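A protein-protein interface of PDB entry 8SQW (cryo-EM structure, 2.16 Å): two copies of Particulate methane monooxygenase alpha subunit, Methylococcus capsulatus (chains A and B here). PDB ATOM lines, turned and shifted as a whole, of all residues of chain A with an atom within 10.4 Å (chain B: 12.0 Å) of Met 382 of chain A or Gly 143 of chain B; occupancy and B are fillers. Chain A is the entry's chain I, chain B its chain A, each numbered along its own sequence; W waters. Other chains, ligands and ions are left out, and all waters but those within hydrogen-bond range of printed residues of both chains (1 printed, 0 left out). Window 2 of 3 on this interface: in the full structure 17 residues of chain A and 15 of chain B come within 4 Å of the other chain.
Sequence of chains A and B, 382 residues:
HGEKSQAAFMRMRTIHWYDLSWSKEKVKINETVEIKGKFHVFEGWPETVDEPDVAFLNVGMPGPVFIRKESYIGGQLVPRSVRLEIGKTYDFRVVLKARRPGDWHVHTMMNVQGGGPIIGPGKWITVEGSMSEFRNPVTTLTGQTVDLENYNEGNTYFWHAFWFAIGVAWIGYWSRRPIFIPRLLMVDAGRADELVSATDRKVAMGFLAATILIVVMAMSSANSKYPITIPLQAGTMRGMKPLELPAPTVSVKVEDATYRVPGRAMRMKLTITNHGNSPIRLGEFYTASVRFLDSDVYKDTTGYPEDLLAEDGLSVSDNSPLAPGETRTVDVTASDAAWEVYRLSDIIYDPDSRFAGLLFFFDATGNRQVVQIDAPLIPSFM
The guanidinium group (NH2) of Arg 260 of chain A lies within hydrogen-bond range of the backbone carbonyl oxygen (O) of Phe 381 of chain A, at 2.7 Å.
The guanidinium group of Arg 260 of chain A lies within hydrogen-bond range of the backbone carbonyl oxygen of Met 382 of chain A (2.4 Å).
N of Tyr 259 of chain A is in hydrogen-bond range of O of Ile 378 of chain A, at 3.3 Å.
OG1 of Thr 142 of chain B sits at hydrogen-bond distance from OG1 of Thr 140 of chain B (2.5 Å).
The side-chain hydroxyl (OG1) of Thr 142 of chain B sits at hydrogen-bond distance from the side-chain amide nitrogen (NE2) of Gln 144 of chain B.
No position is printed for both chains.
Water W1 bridges the backbone carbonyl oxygen of Thr 229 of chain B and the backbone carbonyl oxygen of Ile 348 of chain A.
Among the printed residues, pairs that only touch across the chains: Ile 378 of chain A with Leu 141 of chain B (3.9 Å), Pro 379 of chain A with Leu 141 of chain B (3.6 Å), Phe 381 of chain A with Leu 141 of chain B (3.9 Å), Phe 381 of chain A with Ile 228 of chain B (3.4 Å), Met 382 of chain A with Thr 142 of chain B (3.8 Å) and Met 382 of chain A with Gly 143 of chain B (3.9 Å).
Of the 11 printed residues of chain A, 4 touch a printed residue of chain B.
Among the printed residues, 7 pairs touch across the chains.
Of the printed residues of chain B, Ile 378 of chain A touches Leu 141 (3.9 Å).
Of the printed residues of chain B, Pro 379 of chain A touches Leu 141.
No residue of chain B comes within 4 Å of Ser 380 of chain A.
Printed residues of chain B within 4 Å of Phe 381 of chain A: Leu 141 (3.9 Å) and Ile 228 (3.4 Å).
Met 382 of chain A touches just these residues of chain B: Leu 141 (3.0 Å), Thr 142 (3.8 Å) and Gly 143 (3.9 Å).
Thr 142 of chain B touches one residue of chain A.
No residue of chain A comes within 4 Å of Gln 144 of chain B.
Of the printed residues of chain A, Ile 228 of chain B touches Phe 381.
The nearest residue of chain B that does not touch Met 382 of chain A is Thr 140 of chain B (5.7 Å).
The nearest residue of chain A that does not touch Gly 143 of chain B is Phe 381 of chain A (7.3 Å).
The side-chain sulfur (SD) of Met 382 of chain A sits close to the backbone carbonyl oxygen (O) of Leu 141 of chain B.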
ATOM      1  N   THR A 258      20.381  20.399  30.651  1.00  0.00           N
ATOM      2  CA  THR A 258      19.523  19.788  29.649  1.00  0.00           C
ATOM      3  C   THR A 258      20.027  20.114  28.251  1.00  0.00           C
ATOM      4  O   THR A 258      20.692  21.127  28.030  1.00  0.00           O
ATOM      5  CB  THR A 258      18.064  20.254  29.787  1.00  0.00           C
ATOM      6  OG1 THR A 258      18.004  21.683  29.704  1.00  0.00           O
ATOM      7  CG2 THR A 258      17.471  19.798  31.113  1.00  0.00           C
ATOM      8  N   TYR A 259      19.702  19.230  27.313  1.00  0.00           N
ATOM      9  CA  TYR A 259      19.974  19.444  25.901  1.00  0.00           C
ATOM     10  C   TYR A 259      18.783  18.951  25.097  1.00  0.00           C
ATOM     11  O   TYR A 259      18.183  17.925  25.428  1.00  0.00           O
ATOM     12  CB  TYR A 259      21.257  18.731  25.452  1.00  0.00           C
ATOM     13  CG  TYR A 259      21.170  17.223  25.467  1.00  0.00           C
ATOM     14  CD1 TYR A 259      21.113  16.526  26.662  1.00  0.00           C
ATOM     15  CD2 TYR A 259      21.140  16.499  24.286  1.00  0.00           C
ATOM     16  CE1 TYR A 259      21.037  15.151  26.684  1.00  0.00           C
ATOM     17  CE2 TYR A 259      21.061  15.123  24.296  1.00  0.00           C
ATOM     18  CZ  TYR A 259      21.007  14.456  25.500  1.00  0.00           C
ATOM     19  OH  TYR A 259      20.929  13.084  25.520  1.00  0.00           O
ATOM     20  N   ARG A 260      18.437  19.690  24.048  1.00  0.00           N
ATOM     21  CA  ARG A 260      17.292  19.346  23.220  1.00  0.00           C
ATOM     22  C   ARG A 260      17.635  18.214  22.264  1.00  0.00           C
ATOM     23  O   ARG A 260      18.724  18.176  21.684  1.00  0.00           O
ATOM     24  CB  ARG A 260      16.816  20.566  22.435  1.00  0.00           C
ATOM     25  CG  ARG A 260      16.356  21.720  23.305  1.00  0.00           C
ATOM     26  CD  ARG A 260      14.868  21.628  23.573  1.00  0.00           C
ATOM     27  NE  ARG A 260      14.197  20.771  22.604  1.00  0.00           N
ATOM     28  CZ  ARG A 260      13.100  20.070  22.858  1.00  0.00           C
ATOM     29  NH1 ARG A 260      12.524  20.095  24.049  1.00  0.00           N
ATOM     30  NH2 ARG A 260      12.568  19.327  21.892  1.00  0.00           N
ATOM     31  N   VAL A 261      16.696  17.285  22.107  1.00  0.00           N
ATOM     32  CA  VAL A 261      16.827  16.194  21.145  1.00  0.00           C
ATOM     33  C   VAL A 261      15.696  16.304  20.128  1.00  0.00           C
ATOM     34  O   VAL A 261      14.528  16.086  20.479  1.00  0.00           O
ATOM     35  CB  VAL A 261      16.811  14.825  21.838  1.00  0.00           C
ATOM     36  CG1 VAL A 261      17.167  13.727  20.852  1.00  0.00           C
ATOM     37  CG2 VAL A 261      17.769  14.816  23.017  1.00  0.00           C
ATOM     38  N   PRO A 262      15.985  16.643  18.862  1.00  0.00           N
ATOM     39  CA  PRO A 262      17.317  16.991  18.368  1.00  0.00           C
ATOM     40  C   PRO A 262      17.660  18.456  18.616  1.00  0.00           C
ATOM     41  O   PRO A 262      16.763  19.261  18.867  1.00  0.00           O
ATOM     42  CB  PRO A 262      17.229  16.701  16.862  1.00  0.00           C
ATOM     43  CG  PRO A 262      15.770  16.365  16.579  1.00  0.00           C
ATOM     44  CD  PRO A 262      14.978  16.724  17.792  1.00  0.00           C
ATOM     45  N   ILE A 348      22.678  10.798  24.039  1.00  0.00           N
ATOM     46  CA  ILE A 348      21.413  10.107  24.261  1.00  0.00           C
ATOM     47  C   ILE A 348      21.567   8.609  24.022  1.00  0.00           C
ATOM     48  O   ILE A 348      20.811   7.804  24.579  1.00  0.00           O
ATOM     49  CB  ILE A 348      20.312  10.720  23.375  1.00  0.00           C
ATOM     50  CG1 ILE A 348      18.925  10.300  23.870  1.00  0.00           C
ATOM     51  CG2 ILE A 348      20.514  10.345  21.912  1.00  0.00           C
ATOM     52  CD1 ILE A 348      17.817  10.615  22.901  1.00  0.00           C
ATOM     53  N   ILE A 378      20.325  15.818  31.136  1.00  0.00           N
ATOM     54  CA  ILE A 378      18.982  15.285  30.940  1.00  0.00           C
ATOM     55  C   ILE A 378      18.489  15.716  29.563  1.00  0.00           C
ATOM     56  O   ILE A 378      18.363  16.923  29.316  1.00  0.00           O
ATOM     57  CB  ILE A 378      18.021  15.763  32.038  1.00  0.00           C
ATOM     58  CG1 ILE A 378      18.575  15.412  33.420  1.00  0.00           C
ATOM     59  CG2 ILE A 378      16.647  15.165  31.825  1.00  0.00           C
ATOM     60  CD1 ILE A 378      18.829  13.941  33.624  1.00  0.00           C
ATOM     61  N   PRO A 379      18.197  14.789  28.658  1.00  0.00           N
ATOM     62  CA  PRO A 379      17.610  15.179  27.375  1.00  0.00           C
ATOM     63  C   PRO A 379      16.200  15.716  27.542  1.00  0.00           C
ATOM     64  O   PRO A 379      15.462  15.329  28.452  1.00  0.00           O
ATOM     65  CB  PRO A 379      17.618  13.873  26.573  1.00  0.00           C
ATOM     66  CG  PRO A 379      17.536  12.810  27.618  1.00  0.00           C
ATOM     67  CD  PRO A 379      18.332  13.327  28.785  1.00  0.00           C
ATOM     68  N   SER A 380      15.830  16.627  26.648  1.00  0.00           N
ATOM     69  CA  SER A 380      14.477  17.165  26.580  1.00  0.00           C
ATOM     70  C   SER A 380      13.951  16.962  25.172  1.00  0.00           C
ATOM     71  O   SER A 380      14.647  17.270  24.198  1.00  0.00           O
ATOM     72  CB  SER A 380      14.444  18.647  26.960  1.00  0.00           C
ATOM     73  OG  SER A 380      15.050  19.443  25.959  1.00  0.00           O
ATOM     74  N   PHE A 381      12.729  16.443  25.059  1.00  0.00           N
ATOM     75  CA  PHE A 381      12.172  16.070  23.765  1.00  0.00           C
ATOM     76  C   PHE A 381      10.993  16.936  23.354  1.00  0.00           C
ATOM     77  O   PHE A 381      10.833  17.230  22.166  1.00  0.00           O
ATOM     78  CB  PHE A 381      11.774  14.586  23.785  1.00  0.00           C
ATOM     79  CG  PHE A 381      12.851  13.687  24.321  1.00  0.00           C
ATOM     80  CD1 PHE A 381      13.892  13.273  23.508  1.00  0.00           C
ATOM     81  CD2 PHE A 381      12.830  13.266  25.640  1.00  0.00           C
ATOM     82  CE1 PHE A 381      14.888  12.454  23.999  1.00  0.00           C
ATOM     83  CE2 PHE A 381      13.823  12.447  26.137  1.00  0.00           C
ATOM     84  CZ  PHE A 381      14.852  12.041  25.316  1.00  0.00           C
ATOM     85  N   MET A 382      10.156  17.354  24.299  1.00  0.00           N
ATOM     86  CA  MET A 382       9.067  18.273  23.986  1.00  0.00           C
ATOM     87  C   MET A 382       9.370  19.671  24.513  1.00  0.00           C
ATOM     88  O   MET A 382      10.387  19.892  25.166  1.00  0.00           O
ATOM     89  CB  MET A 382       7.738  17.774  24.564  1.00  0.00           C
ATOM     90  CG  MET A 382       7.528  16.275  24.451  1.00  0.00           C
ATOM     91  SD  MET A 382       8.225  15.384  25.850  1.00  0.00           S
ATOM     92  CE  MET A 382       7.189  15.980  27.184  1.00  0.00           C
ATOM     93  N   PRO B 137       3.903   5.352  41.074  1.00  0.00           N
ATOM     94  CA  PRO B 137       3.823   6.189  39.875  1.00  0.00           C
ATOM     95  C   PRO B 137       5.174   6.785  39.520  1.00  0.00           C
ATOM     96  O   PRO B 137       6.024   7.016  40.383  1.00  0.00           O
ATOM     97  CB  PRO B 137       2.822   7.280  40.274  1.00  0.00           C
ATOM     98  CG  PRO B 137       2.970   7.387  41.744  1.00  0.00           C
ATOM     99  CD  PRO B 137       3.287   6.003  42.243  1.00  0.00           C
ATOM    100  N   VAL B 138       5.364   7.031  38.228  1.00  0.00           N
ATOM    101  CA  VAL B 138       6.562   7.703  37.736  1.00  0.00           C
ATOM    102  C   VAL B 138       6.199   8.430  36.451  1.00  0.00           C
ATOM    103  O   VAL B 138       5.370   7.954  35.669  1.00  0.00           O
ATOM    104  CB  VAL B 138       7.730   6.717  37.524  1.00  0.00           C
ATOM    105  CG1 VAL B 138       7.471   5.798  36.342  1.00  0.00           C
ATOM    106  CG2 VAL B 138       9.037   7.472  37.348  1.00  0.00           C
ATOM    107  N   THR B 139       6.795   9.599  36.245  1.00  0.00           N
ATOM    108  CA  THR B 139       6.545  10.392  35.051  1.00  0.00           C
ATOM    109  C   THR B 139       7.782  10.380  34.166  1.00  0.00           C
ATOM    110  O   THR B 139       8.886  10.702  34.617  1.00  0.00           O
ATOM    111  CB  THR B 139       6.173  11.828  35.420  1.00  0.00           C
ATOM    112  OG1 THR B 139       5.017  11.821  36.267  1.00  0.00           O
ATOM    113  CG2 THR B 139       5.875  12.640  34.171  1.00  0.00           C
ATOM    114  N   THR B 140       7.595  10.014  32.905  1.00  0.00           N
ATOM    115  CA  THR B 140       8.694   9.917  31.961  1.00  0.00           C
ATOM    116  C   THR B 140       8.951  11.264  31.295  1.00  0.00           C
ATOM    117  O   THR B 140       8.146  12.196  31.379  1.00  0.00           O
ATOM    118  CB  THR B 140       8.403   8.851  30.905  1.00  0.00           C
ATOM    119  OG1 THR B 140       7.461   9.366  29.960  1.00  0.00           O
ATOM    120  CG2 THR B 140       7.824   7.606  31.556  1.00  0.00           C
ATOM    121  N   LEU B 141      10.096  11.361  30.622  1.00  0.00           N
ATOM    122  CA  LEU B 141      10.414  12.561  29.860  1.00  0.00           C
ATOM    123  C   LEU B 141       9.568  12.693  28.603  1.00  0.00           C
ATOM    124  O   LEU B 141       9.614  13.744  27.953  1.00  0.00           O
ATOM    125  CB  LEU B 141      11.898  12.578  29.498  1.00  0.00           C
ATOM    126  CG  LEU B 141      12.843  12.860  30.666  1.00  0.00           C
ATOM    127  CD1 LEU B 141      14.264  12.478  30.312  1.00  0.00           C
ATOM    128  CD2 LEU B 141      12.767  14.323  31.071  1.00  0.00           C
ATOM    129  N   THR B 142       8.805  11.660  28.247  1.00  0.00           N
ATOM    130  CA  THR B 142       7.875  11.740  27.131  1.00  0.00           C
ATOM    131  C   THR B 142       6.496  12.230  27.554  1.00  0.00           C
ATOM    132  O   THR B 142       5.586  12.267  26.720  1.00  0.00           O
ATOM    133  CB  THR B 142       7.741  10.376  26.452  1.00  0.00           C
ATOM    134  OG1 THR B 142       7.544   9.364  27.446  1.00  0.00           O
ATOM    135  CG2 THR B 142       8.999  10.056  25.662  1.00  0.00           C
ATOM    136  N   GLY B 143       6.320  12.593  28.824  1.00  0.00           N
ATOM    137  CA  GLY B 143       5.081  13.188  29.278  1.00  0.00           C
ATOM    138  C   GLY B 143       3.963  12.227  29.607  1.00  0.00           C
ATOM    139  O   GLY B 143       2.790  12.589  29.462  1.00  0.00           O
ATOM    140  N   GLN B 144       4.280  11.016  30.053  1.00  0.00           N
ATOM    141  CA  GLN B 144       3.257  10.062  30.456  1.00  0.00           C
ATOM    142  C   GLN B 144       3.570   9.541  31.848  1.00  0.00           C
ATOM    143  O   GLN B 144       4.736   9.327  32.193  1.00  0.00           O
ATOM    144  CB  GLN B 144       3.152   8.894  29.469  1.00  0.00           C
ATOM    145  CG  GLN B 144       4.483   8.406  28.929  1.00  0.00           C
ATOM    146  CD  GLN B 144       4.406   8.034  27.463  1.00  0.00           C
ATOM    147  OE1 GLN B 144       3.653   8.635  26.697  1.00  0.00           O
ATOM    148  NE2 GLN B 144       5.187   7.039  27.061  1.00  0.00           N
ATOM    149  N   THR B 145       2.524   9.341  32.644  1.00  0.00           N
ATOM    150  CA  THR B 145       2.651   8.826  33.999  1.00  0.00           C
ATOM    151  C   THR B 145       2.200   7.372  34.014  1.00  0.00           C
ATOM    152  O   THR B 145       1.080   7.061  33.595  1.00  0.00           O
ATOM    153  CB  THR B 145       1.821   9.653  34.981  1.00  0.00           C
ATOM    154  OG1 THR B 145       2.331  10.990  35.031  1.00  0.00           O
ATOM    155  CG2 THR B 145       1.882   9.040  36.374  1.00  0.00           C
ATOM    156  N   VAL B 146       3.068   6.488  34.498  1.00  0.00           N
ATOM    157  CA  VAL B 146       2.785   5.061  34.536  1.00  0.00           C
ATOM    158  C   VAL B 146       2.994   4.553  35.954  1.00  0.00           C
ATOM    159  O   VAL B 146       3.725   5.151  36.748  1.00  0.00           O
ATOM    160  CB  VAL B 146       3.661   4.269  33.536  1.00  0.00           C
ATOM    161  CG1 VAL B 146       3.647   4.929  32.169  1.00  0.00           C
ATOM    162  CG2 VAL B 146       5.087   4.144  34.051  1.00  0.00           C
ATOM    163  N   ASP B 147       2.331   3.447  36.269  1.00  0.00           N
ATOM    164  CA  ASP B 147       2.526   2.767  37.539  1.00  0.00           C
ATOM    165  C   ASP B 147       3.472   1.592  37.334  1.00  0.00           C
ATOM    166  O   ASP B 147       3.170   0.662  36.580  1.00  0.00           O
ATOM    167  CB  ASP B 147       1.192   2.284  38.109  1.00  0.00           C
ATOM    168  CG  ASP B 147       1.288   1.869  39.569  1.00  0.00           C
ATOM    169  OD1 ASP B 147       2.382   1.473  40.020  1.00  0.00           O
ATOM    170  OD2 ASP B 147       0.257   1.936  40.272  1.00  0.00           O
ATOM    171  N   TYR B 151       3.001  -1.587  34.769  1.00  0.00           N
ATOM    172  CA  TYR B 151       3.360  -1.057  33.459  1.00  0.00           C
ATOM    173  C   TYR B 151       4.061  -2.126  32.631  1.00  0.00           C
ATOM    174  O   TYR B 151       4.951  -2.824  33.127  1.00  0.00           O
ATOM    175  CB  TYR B 151       4.253   0.170  33.623  1.00  0.00           C
ATOM    176  CG  TYR B 151       4.877   0.681  32.349  1.00  0.00           C
ATOM    177  CD1 TYR B 151       4.130   1.411  31.436  1.00  0.00           C
ATOM    178  CD2 TYR B 151       6.215   0.449  32.066  1.00  0.00           C
ATOM    179  CE1 TYR B 151       4.697   1.889  30.275  1.00  0.00           C
ATOM    180  CE2 TYR B 151       6.790   0.921  30.905  1.00  0.00           C
ATOM    181  CZ  TYR B 151       6.027   1.642  30.015  1.00  0.00           C
ATOM    182  OH  TYR B 151       6.593   2.118  28.858  1.00  0.00           O
ATOM    183  N   TYR B 226       6.840   4.366  21.202  1.00  0.00           N
ATOM    184  CA  TYR B 226       8.054   4.603  21.977  1.00  0.00           C
ATOM    185  C   TYR B 226       9.222   4.990  21.066  1.00  0.00           C
ATOM    186  O   TYR B 226      10.249   4.307  21.045  1.00  0.00           O
ATOM    187  CB  TYR B 226       8.415   3.388  22.818  1.00  0.00           C
ATOM    188  CG  TYR B 226       7.239   2.678  23.439  1.00  0.00           C
ATOM    189  CD1 TYR B 226       6.562   3.225  24.518  1.00  0.00           C
ATOM    190  CD2 TYR B 226       6.804   1.459  22.940  1.00  0.00           C
ATOM    191  CE1 TYR B 226       5.485   2.577  25.084  1.00  0.00           C
ATOM    192  CE2 TYR B 226       5.727   0.807  23.499  1.00  0.00           C
ATOM    193  CZ  TYR B 226       5.073   1.369  24.573  1.00  0.00           C
ATOM    194  OH  TYR B 226       4.000   0.720  25.135  1.00  0.00           O
ATOM    195  N   PRO B 227       9.096   6.073  20.289  1.00  0.00           N
ATOM    196  CA  PRO B 227      10.206   6.462  19.410  1.00  0.00           C
ATOM    197  C   PRO B 227      11.429   6.943  20.167  1.00  0.00           C
ATOM    198  O   PRO B 227      12.517   7.000  19.582  1.00  0.00           O
ATOM    199  CB  PRO B 227       9.602   7.581  18.556  1.00  0.00           C
ATOM    200  CG  PRO B 227       8.563   8.183  19.429  1.00  0.00           C
ATOM    201  CD  PRO B 227       8.015   7.076  20.287  1.00  0.00           C
ATOM    202  N   ILE B 228      11.284   7.289  21.441  1.00  0.00           N
ATOM    203  CA  ILE B 228      12.377   7.793  22.257  1.00  0.00           C
ATOM    204  C   ILE B 228      12.703   6.733  23.301  1.00  0.00           C
ATOM    205  O   ILE B 228      11.904   6.474  24.208  1.00  0.00           O
ATOM    206  CB  ILE B 228      12.023   9.130  22.919  1.00  0.00           C
ATOM    207  CG1 ILE B 228      11.883  10.228  21.860  1.00  0.00           C
ATOM    208  CG2 ILE B 228      13.066   9.503  23.944  1.00  0.00           C
ATOM    209  CD1 ILE B 228      10.554  10.940  21.901  1.00  0.00           C
ATOM    210  N   THR B 229      13.873   6.118  23.174  1.00  0.00           N
ATOM    211  CA  THR B 229      14.357   5.143  24.137  1.00  0.00           C
ATOM    212  C   THR B 229      15.821   5.421  24.444  1.00  0.00           C
ATOM    213  O   THR B 229      16.552   5.972  23.618  1.00  0.00           O
ATOM    214  CB  THR B 229      14.204   3.694  23.635  1.00  0.00           C
ATOM    215  OG1 THR B 229      14.949   3.521  22.425  1.00  0.00           O
ATOM    216  CG2 THR B 229      12.744   3.349  23.393  1.00  0.00           C
HETATM  217  O   HOH W   1      18.956   6.535  22.819  1.00  0.00           O
